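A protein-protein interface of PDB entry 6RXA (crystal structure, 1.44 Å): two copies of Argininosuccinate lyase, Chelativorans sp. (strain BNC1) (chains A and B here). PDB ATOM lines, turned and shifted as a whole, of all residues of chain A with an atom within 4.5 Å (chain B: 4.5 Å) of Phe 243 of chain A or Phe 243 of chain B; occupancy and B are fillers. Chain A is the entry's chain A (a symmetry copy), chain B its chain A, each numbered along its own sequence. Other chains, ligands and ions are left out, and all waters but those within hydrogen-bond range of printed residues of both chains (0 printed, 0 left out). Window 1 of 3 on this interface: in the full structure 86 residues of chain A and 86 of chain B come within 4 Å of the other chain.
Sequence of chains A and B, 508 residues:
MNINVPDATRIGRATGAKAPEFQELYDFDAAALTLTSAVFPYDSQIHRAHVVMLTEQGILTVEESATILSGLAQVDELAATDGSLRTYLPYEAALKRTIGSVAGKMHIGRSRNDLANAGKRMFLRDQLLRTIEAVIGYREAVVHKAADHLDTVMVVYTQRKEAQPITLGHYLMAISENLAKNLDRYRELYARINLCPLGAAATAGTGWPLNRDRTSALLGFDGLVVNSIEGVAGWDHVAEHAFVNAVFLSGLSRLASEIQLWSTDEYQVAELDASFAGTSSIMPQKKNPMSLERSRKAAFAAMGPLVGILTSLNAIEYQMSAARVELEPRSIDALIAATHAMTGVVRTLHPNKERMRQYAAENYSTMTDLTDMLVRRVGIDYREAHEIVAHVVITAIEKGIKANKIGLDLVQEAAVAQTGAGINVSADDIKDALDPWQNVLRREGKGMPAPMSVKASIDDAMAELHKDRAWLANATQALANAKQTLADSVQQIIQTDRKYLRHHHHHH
Ala 239 of chain A touches Phe 243 of chain B, and with the chains exchanged Phe 243 of chain A touches Ala 239 of chain B. Phe 243 of chain B touches its own counterpart, Phe 243 of chain A. Val 247 of chain A touches Leu 310 of chain B, and with the chains exchanged Leu 310 of chain A touches Val 247 of chain B. Leu 306 of chain A touches Leu 310 of chain B, and with the chains exchanged Leu 310 of chain A touches Leu 306 of chain B. Positions printed for both chains: 239, 240, 241, 242, 243, 244, 245, 246, 247, 306 and 310. Of the 9 pairs that touch across the chains among the printed residues, 9 have their exchanged pair printed and touching as well.
Among the printed residues, pairs that only touch across the chains: Phe 243 of chain A with Phe 243 of chain B (3.5 Å), Phe 243 of chain A with Glu 240 of chain B (3.5 Å), Glu 240 of chain A with Phe 243 of chain B (3.5 Å), Leu 310 of chain A with Leu 306 of chain B (3.5 Å), Leu 306 of chain A with Leu 310 of chain B (3.5 Å), Ala 239 of chain A with Phe 243 of chain B (3.7 Å), Phe 243 of chain A with Ala 239 of chain B (3.7 Å), Leu 310 of chain A with Val 247 of chain B (3.9 Å) and Val 247 of chain A with Leu 310 of chain B (3.9 Å).
Phe 243 of chain A touches three residues of chain B. Printed residues of chain A within 4 Å of Phe 243 of chain B: Ala 239 (3.7 Å), Glu 240 (3.5 Å) and Phe 243 (3.5 Å). Of the printed residues of chain B, Leu 310 of chain A touches Val 247 (3.9 Å) and Leu 306 (3.5 Å). Printed residues of chain A within 4 Å of Glu 240 of chain B: Phe 243. Of the printed residues of chain B, Ala 239 of chain A touches Phe 243. Of the printed residues of chain B, Val 247 of chain A touches Leu 310. Of the printed residues of chain A, Leu 306 of chain B touches Leu 310 (3.5 Å). His 241 of chain B touches none of the printed residues of chain A. The nearest residue of chain B that does not touch Phe 243 of chain A is Leu 306 of chain B (4.1 Å). The nearest residue of chain A that does not touch Phe 243 of chain B is Leu 306 of chain A (4.1 Å). The nearest printed residue of chain A that does not touch Glu 240 of chain B is Val 247 of chain A (5.4 Å).
Of the 11 printed residues of chain B, 6 touch a printed residue of chain A. Hydrophobic or aromatic side chains of chain B within 4 Å of the printed part of chain A: Phe 243, Leu 306 and Leu 310. Of the 11 printed residues of chain A, 6 touch a printed residue of chain B. Hydrophobic or aromatic side chains of chain A within 4 Å of the printed part of chain B: Phe 243, Leu 306 and Leu 310.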
ATOM      1  N   ALA A 239      24.844   6.175  12.418  1.00  0.00           N
ATOM      2  CA  ALA A 239      24.780   7.556  11.958  1.00  0.00           C
ATOM      3  C   ALA A 239      26.147   8.044  11.498  1.00  0.00           C
ATOM      4  O   ALA A 239      26.257   8.707  10.456  1.00  0.00           O
ATOM      5  CB  ALA A 239      24.245   8.450  13.077  1.00  0.00           C
ATOM      6  N   GLU A 240      27.204   7.711  12.250  1.00  0.00           N
ATOM      7  CA  GLU A 240      28.538   8.180  11.902  1.00  0.00           C
ATOM      8  C   GLU A 240      29.032   7.556  10.601  1.00  0.00           C
ATOM      9  O   GLU A 240      29.661   8.238   9.786  1.00  0.00           O
ATOM     10  CB  GLU A 240      29.516   7.925  13.045  1.00  0.00           C
ATOM     11  CG  GLU A 240      30.890   8.498  12.808  1.00  0.00           C
ATOM     12  CD  GLU A 240      31.867   8.198  13.926  1.00  0.00           C
ATOM     13  OE1 GLU A 240      31.461   7.699  14.984  1.00  0.00           O
ATOM     14  OE2 GLU A 240      33.062   8.468  13.742  1.00  0.00           O
ATOM     15  N   HIS A 241      28.747   6.275  10.383  1.00  0.00           N
ATOM     16  CA  HIS A 241      29.098   5.635   9.113  1.00  0.00           C
ATOM     17  C   HIS A 241      28.397   6.329   7.946  1.00  0.00           C
ATOM     18  O   HIS A 241      29.026   6.648   6.923  1.00  0.00           O
ATOM     19  CB  HIS A 241      28.738   4.152   9.223  1.00  0.00           C
ATOM     20  CG  HIS A 241      29.351   3.293   8.172  1.00  0.00           C
ATOM     21  ND1 HIS A 241      29.488   1.929   8.325  1.00  0.00           N
ATOM     22  CD2 HIS A 241      29.847   3.589   6.947  1.00  0.00           C
ATOM     23  CE1 HIS A 241      30.049   1.424   7.240  1.00  0.00           C
ATOM     24  NE2 HIS A 241      30.275   2.409   6.388  1.00  0.00           N
ATOM     25  N   ALA A 242      27.112   6.629   8.102  1.00  0.00           N
ATOM     26  CA  ALA A 242      26.388   7.366   7.076  1.00  0.00           C
ATOM     27  C   ALA A 242      27.001   8.743   6.846  1.00  0.00           C
ATOM     28  O   ALA A 242      27.104   9.204   5.695  1.00  0.00           O
ATOM     29  CB  ALA A 242      24.914   7.489   7.460  1.00  0.00           C
ATOM     30  N   PHE A 243      27.416   9.419   7.919  1.00  0.00           N
ATOM     31  CA  PHE A 243      28.012  10.735   7.749  1.00  0.00           C
ATOM     32  C   PHE A 243      29.345  10.675   7.006  1.00  0.00           C
ATOM     33  O   PHE A 243      29.599  11.484   6.101  1.00  0.00           O
ATOM     34  CB  PHE A 243      28.245  11.452   9.073  1.00  0.00           C
ATOM     35  CG  PHE A 243      29.109  12.654   8.893  1.00  0.00           C
ATOM     36  CD1 PHE A 243      28.611  13.784   8.243  1.00  0.00           C
ATOM     37  CD2 PHE A 243      30.427  12.646   9.284  1.00  0.00           C
ATOM     38  CE1 PHE A 243      29.403  14.872   8.019  1.00  0.00           C
ATOM     39  CE2 PHE A 243      31.230  13.752   9.064  1.00  0.00           C
ATOM     40  CZ  PHE A 243      30.717  14.863   8.414  1.00  0.00           C
ATOM     41  N   VAL A 244      30.258   9.784   7.420  1.00  0.00           N
ATOM     42  CA  VAL A 244      31.559   9.781   6.759  1.00  0.00           C
ATOM     43  C   VAL A 244      31.372   9.469   5.275  1.00  0.00           C
ATOM     44  O   VAL A 244      32.007  10.083   4.408  1.00  0.00           O
ATOM     45  CB  VAL A 244      32.578   8.851   7.443  1.00  0.00           C
ATOM     46  CG1 VAL A 244      33.938   9.007   6.748  1.00  0.00           C
ATOM     47  CG2 VAL A 244      32.700   9.183   8.916  1.00  0.00           C
ATOM     48  N   ASN A 245      30.459   8.543   4.960  1.00  0.00           N
ATOM     49  CA  ASN A 245      30.148   8.276   3.558  1.00  0.00           C
ATOM     50  C   ASN A 245      29.700   9.555   2.856  1.00  0.00           C
ATOM     51  O   ASN A 245      30.143   9.857   1.741  1.00  0.00           O
ATOM     52  CB  ASN A 245      29.046   7.225   3.443  1.00  0.00           C
ATOM     53  CG  ASN A 245      29.502   5.813   3.747  1.00  0.00           C
ATOM     54  OD1 ASN A 245      30.662   5.547   4.091  1.00  0.00           O
ATOM     55  ND2 ASN A 245      28.557   4.879   3.627  1.00  0.00           N
ATOM     56  N   ALA A 246      28.803  10.316   3.485  1.00  0.00           N
ATOM     57  CA  ALA A 246      28.273  11.509   2.836  1.00  0.00           C
ATOM     58  C   ALA A 246      29.355  12.568   2.636  1.00  0.00           C
ATOM     59  O   ALA A 246      29.416  13.212   1.583  1.00  0.00           O
ATOM     60  CB  ALA A 246      27.112  12.099   3.623  1.00  0.00           C
ATOM     61  N   VAL A 247      30.184  12.810   3.656  1.00  0.00           N
ATOM     62  CA  VAL A 247      31.190  13.869   3.511  1.00  0.00           C
ATOM     63  C   VAL A 247      32.287  13.463   2.530  1.00  0.00           C
ATOM     64  O   VAL A 247      32.700  14.259   1.676  1.00  0.00           O
ATOM     65  CB  VAL A 247      31.727  14.371   4.870  1.00  0.00           C
ATOM     66  CG1 VAL A 247      32.726  13.403   5.479  1.00  0.00           C
ATOM     67  CG2 VAL A 247      32.361  15.764   4.687  1.00  0.00           C
ATOM     68  N   LEU A 306      21.814   9.322   5.908  1.00  0.00           N
ATOM     69  CA  LEU A 306      22.265  10.155   7.019  1.00  0.00           C
ATOM     70  C   LEU A 306      21.088  10.839   7.709  1.00  0.00           C
ATOM     71  O   LEU A 306      20.953  10.787   8.939  1.00  0.00           O
ATOM     72  CB  LEU A 306      23.266  11.188   6.508  1.00  0.00           C
ATOM     73  CG  LEU A 306      23.754  12.239   7.511  1.00  0.00           C
ATOM     74  CD1 LEU A 306      24.396  11.571   8.708  1.00  0.00           C
ATOM     75  CD2 LEU A 306      24.690  13.212   6.814  1.00  0.00           C
ATOM     76  N   LEU A 310      19.493   9.841  11.509  1.00  0.00           N
ATOM     77  CA  LEU A 310      19.467  10.855  12.563  1.00  0.00           C
ATOM     78  C   LEU A 310      18.043  11.235  12.955  1.00  0.00           C
ATOM     79  O   LEU A 310      17.765  11.462  14.141  1.00  0.00           O
ATOM     80  CB  LEU A 310      20.244  12.099  12.152  1.00  0.00           C
ATOM     81  CG  LEU A 310      21.760  11.978  12.254  1.00  0.00           C
ATOM     82  CD1 LEU A 310      22.419  13.135  11.501  1.00  0.00           C
ATOM     83  CD2 LEU A 310      22.257  11.911  13.682  1.00  0.00           C
ATOM     84  N   ALA B 239      31.407  20.585   8.001  1.00  0.00           N
ATOM     85  CA  ALA B 239      30.402  19.533   7.943  1.00  0.00           C
ATOM     86  C   ALA B 239      30.531  18.586   9.128  1.00  0.00           C
ATOM     87  O   ALA B 239      29.520  18.199   9.733  1.00  0.00           O
ATOM     88  CB  ALA B 239      30.536  18.762   6.629  1.00  0.00           C
ATOM     89  N   GLU B 240      31.767  18.216   9.487  1.00  0.00           N
ATOM     90  CA  GLU B 240      31.969  17.274  10.581  1.00  0.00           C
ATOM     91  C   GLU B 240      31.558  17.874  11.921  1.00  0.00           C
ATOM     92  O   GLU B 240      30.966  17.180  12.755  1.00  0.00           O
ATOM     93  CB  GLU B 240      33.415  16.786  10.613  1.00  0.00           C
ATOM     94  CG  GLU B 240      33.670  15.713  11.639  1.00  0.00           C
ATOM     95  CD  GLU B 240      35.118  15.269  11.697  1.00  0.00           C
ATOM     96  OE1 GLU B 240      35.914  15.648  10.829  1.00  0.00           O
ATOM     97  OE2 GLU B 240      35.462  14.527  12.627  1.00  0.00           O
ATOM     98  N   HIS B 241      31.846  19.154  12.141  1.00  0.00           N
ATOM     99  CA  HIS B 241      31.393  19.825  13.361  1.00  0.00           C
ATOM    100  C   HIS B 241      29.867  19.814  13.449  1.00  0.00           C
ATOM    101  O   HIS B 241      29.291  19.479  14.497  1.00  0.00           O
ATOM    102  CB  HIS B 241      31.976  21.240  13.360  1.00  0.00           C
ATOM    103  CG  HIS B 241      31.915  21.929  14.679  1.00  0.00           C
ATOM    104  ND1 HIS B 241      32.725  23.002  14.984  1.00  0.00           N
ATOM    105  CD2 HIS B 241      31.134  21.720  15.765  1.00  0.00           C
ATOM    106  CE1 HIS B 241      32.450  23.419  16.208  1.00  0.00           C
ATOM    107  NE2 HIS B 241      31.487  22.661  16.703  1.00  0.00           N
ATOM    108  N   ALA B 242      29.194  20.115  12.343  1.00  0.00           N
ATOM    109  CA  ALA B 242      27.739  20.046  12.314  1.00  0.00           C
ATOM    110  C   ALA B 242      27.245  18.633  12.601  1.00  0.00           C
ATOM    111  O   ALA B 242      26.244  18.447  13.317  1.00  0.00           O
ATOM    112  CB  ALA B 242      27.219  20.535  10.962  1.00  0.00           C
ATOM    113  N   PHE B 243      27.925  17.621  12.059  1.00  0.00           N
ATOM    114  CA  PHE B 243      27.495  16.254  12.309  1.00  0.00           C
ATOM    115  C   PHE B 243      27.653  15.856  13.775  1.00  0.00           C
ATOM    116  O   PHE B 243      26.747  15.248  14.364  1.00  0.00           O
ATOM    117  CB  PHE B 243      28.247  15.235  11.463  1.00  0.00           C
ATOM    118  CG  PHE B 243      27.997  13.844  11.941  1.00  0.00           C
ATOM    119  CD1 PHE B 243      26.750  13.250  11.744  1.00  0.00           C
ATOM    120  CD2 PHE B 243      28.951  13.155  12.651  1.00  0.00           C
ATOM    121  CE1 PHE B 243      26.484  12.000  12.223  1.00  0.00           C
ATOM    122  CE2 PHE B 243      28.685  11.885  13.131  1.00  0.00           C
ATOM    123  CZ  PHE B 243      27.439  11.314  12.928  1.00  0.00           C
ATOM    124  N   VAL B 244      28.827  16.107  14.373  1.00  0.00           N
ATOM    125  CA  VAL B 244      29.003  15.657  15.750  1.00  0.00           C
ATOM    126  C   VAL B 244      27.970  16.344  16.642  1.00  0.00           C
ATOM    127  O   VAL B 244      27.374  15.717  17.528  1.00  0.00           O
ATOM    128  CB  VAL B 244      30.445  15.832  16.259  1.00  0.00           C
ATOM    129  CG1 VAL B 244      30.553  15.225  17.666  1.00  0.00           C
ATOM    130  CG2 VAL B 244      31.428  15.161  15.322  1.00  0.00           C
ATOM    131  N   ASN B 245      27.707  17.630  16.387  1.00  0.00           N
ATOM    132  CA  ASN B 245      26.651  18.317  17.126  1.00  0.00           C
ATOM    133  C   ASN B 245      25.322  17.583  16.967  1.00  0.00           C
ATOM    134  O   ASN B 245      24.592  17.369  17.943  1.00  0.00           O
ATOM    135  CB  ASN B 245      26.495  19.753  16.631  1.00  0.00           C
ATOM    136  CG  ASN B 245      27.599  20.687  17.084  1.00  0.00           C
ATOM    137  OD1 ASN B 245      28.558  20.303  17.768  1.00  0.00           O
ATOM    138  ND2 ASN B 245      27.466  21.951  16.682  1.00  0.00           N
ATOM    139  N   ALA B 246      24.976  17.203  15.736  1.00  0.00           N
ATOM    140  CA  ALA B 246      23.686  16.569  15.501  1.00  0.00           C
ATOM    141  C   ALA B 246      23.596  15.206  16.183  1.00  0.00           C
ATOM    142  O   ALA B 246      22.562  14.860  16.764  1.00  0.00           O
ATOM    143  CB  ALA B 246      23.401  16.422  14.013  1.00  0.00           C
ATOM    144  N   VAL B 247      24.646  14.387  16.074  1.00  0.00           N
ATOM    145  CA  VAL B 247      24.560  13.045  16.664  1.00  0.00           C
ATOM    146  C   VAL B 247      24.585  13.108  18.190  1.00  0.00           C
ATOM    147  O   VAL B 247      23.802  12.424  18.865  1.00  0.00           O
ATOM    148  CB  VAL B 247      25.590  12.063  16.067  1.00  0.00           C
ATOM    149  CG1 VAL B 247      26.986  12.296  16.617  1.00  0.00           C
ATOM    150  CG2 VAL B 247      25.134  10.615  16.335  1.00  0.00           C
ATOM    151  N   LEU B 306      23.676  20.740   9.294  1.00  0.00           N
ATOM    152  CA  LEU B 306      24.330  19.569   8.719  1.00  0.00           C
ATOM    153  C   LEU B 306      23.923  19.371   7.261  1.00  0.00           C
ATOM    154  O   LEU B 306      24.776  19.202   6.379  1.00  0.00           O
ATOM    155  CB  LEU B 306      23.985  18.334   9.547  1.00  0.00           C
ATOM    156  CG  LEU B 306      24.478  16.983   9.020  1.00  0.00           C
ATOM    157  CD1 LEU B 306      25.983  16.991   8.864  1.00  0.00           C
ATOM    158  CD2 LEU B 306      23.992  15.871   9.936  1.00  0.00           C
ATOM    159  N   LEU B 310      26.351  20.113   3.864  1.00  0.00           N
ATOM    160  CA  LEU B 310      26.639  19.019   2.937  1.00  0.00           C
ATOM    161  C   LEU B 310      26.031  19.262   1.560  1.00  0.00           C
ATOM    162  O   LEU B 310      26.651  18.931   0.540  1.00  0.00           O
ATOM    163  CB  LEU B 310      26.157  17.685   3.491  1.00  0.00           C
ATOM    164  CG  LEU B 310      27.052  17.065   4.558  1.00  0.00           C
ATOM    165  CD1 LEU B 310      26.301  15.937   5.267  1.00  0.00           C
ATOM    166  CD2 LEU B 310      28.376  16.573   4.013  1.00  0.00           C
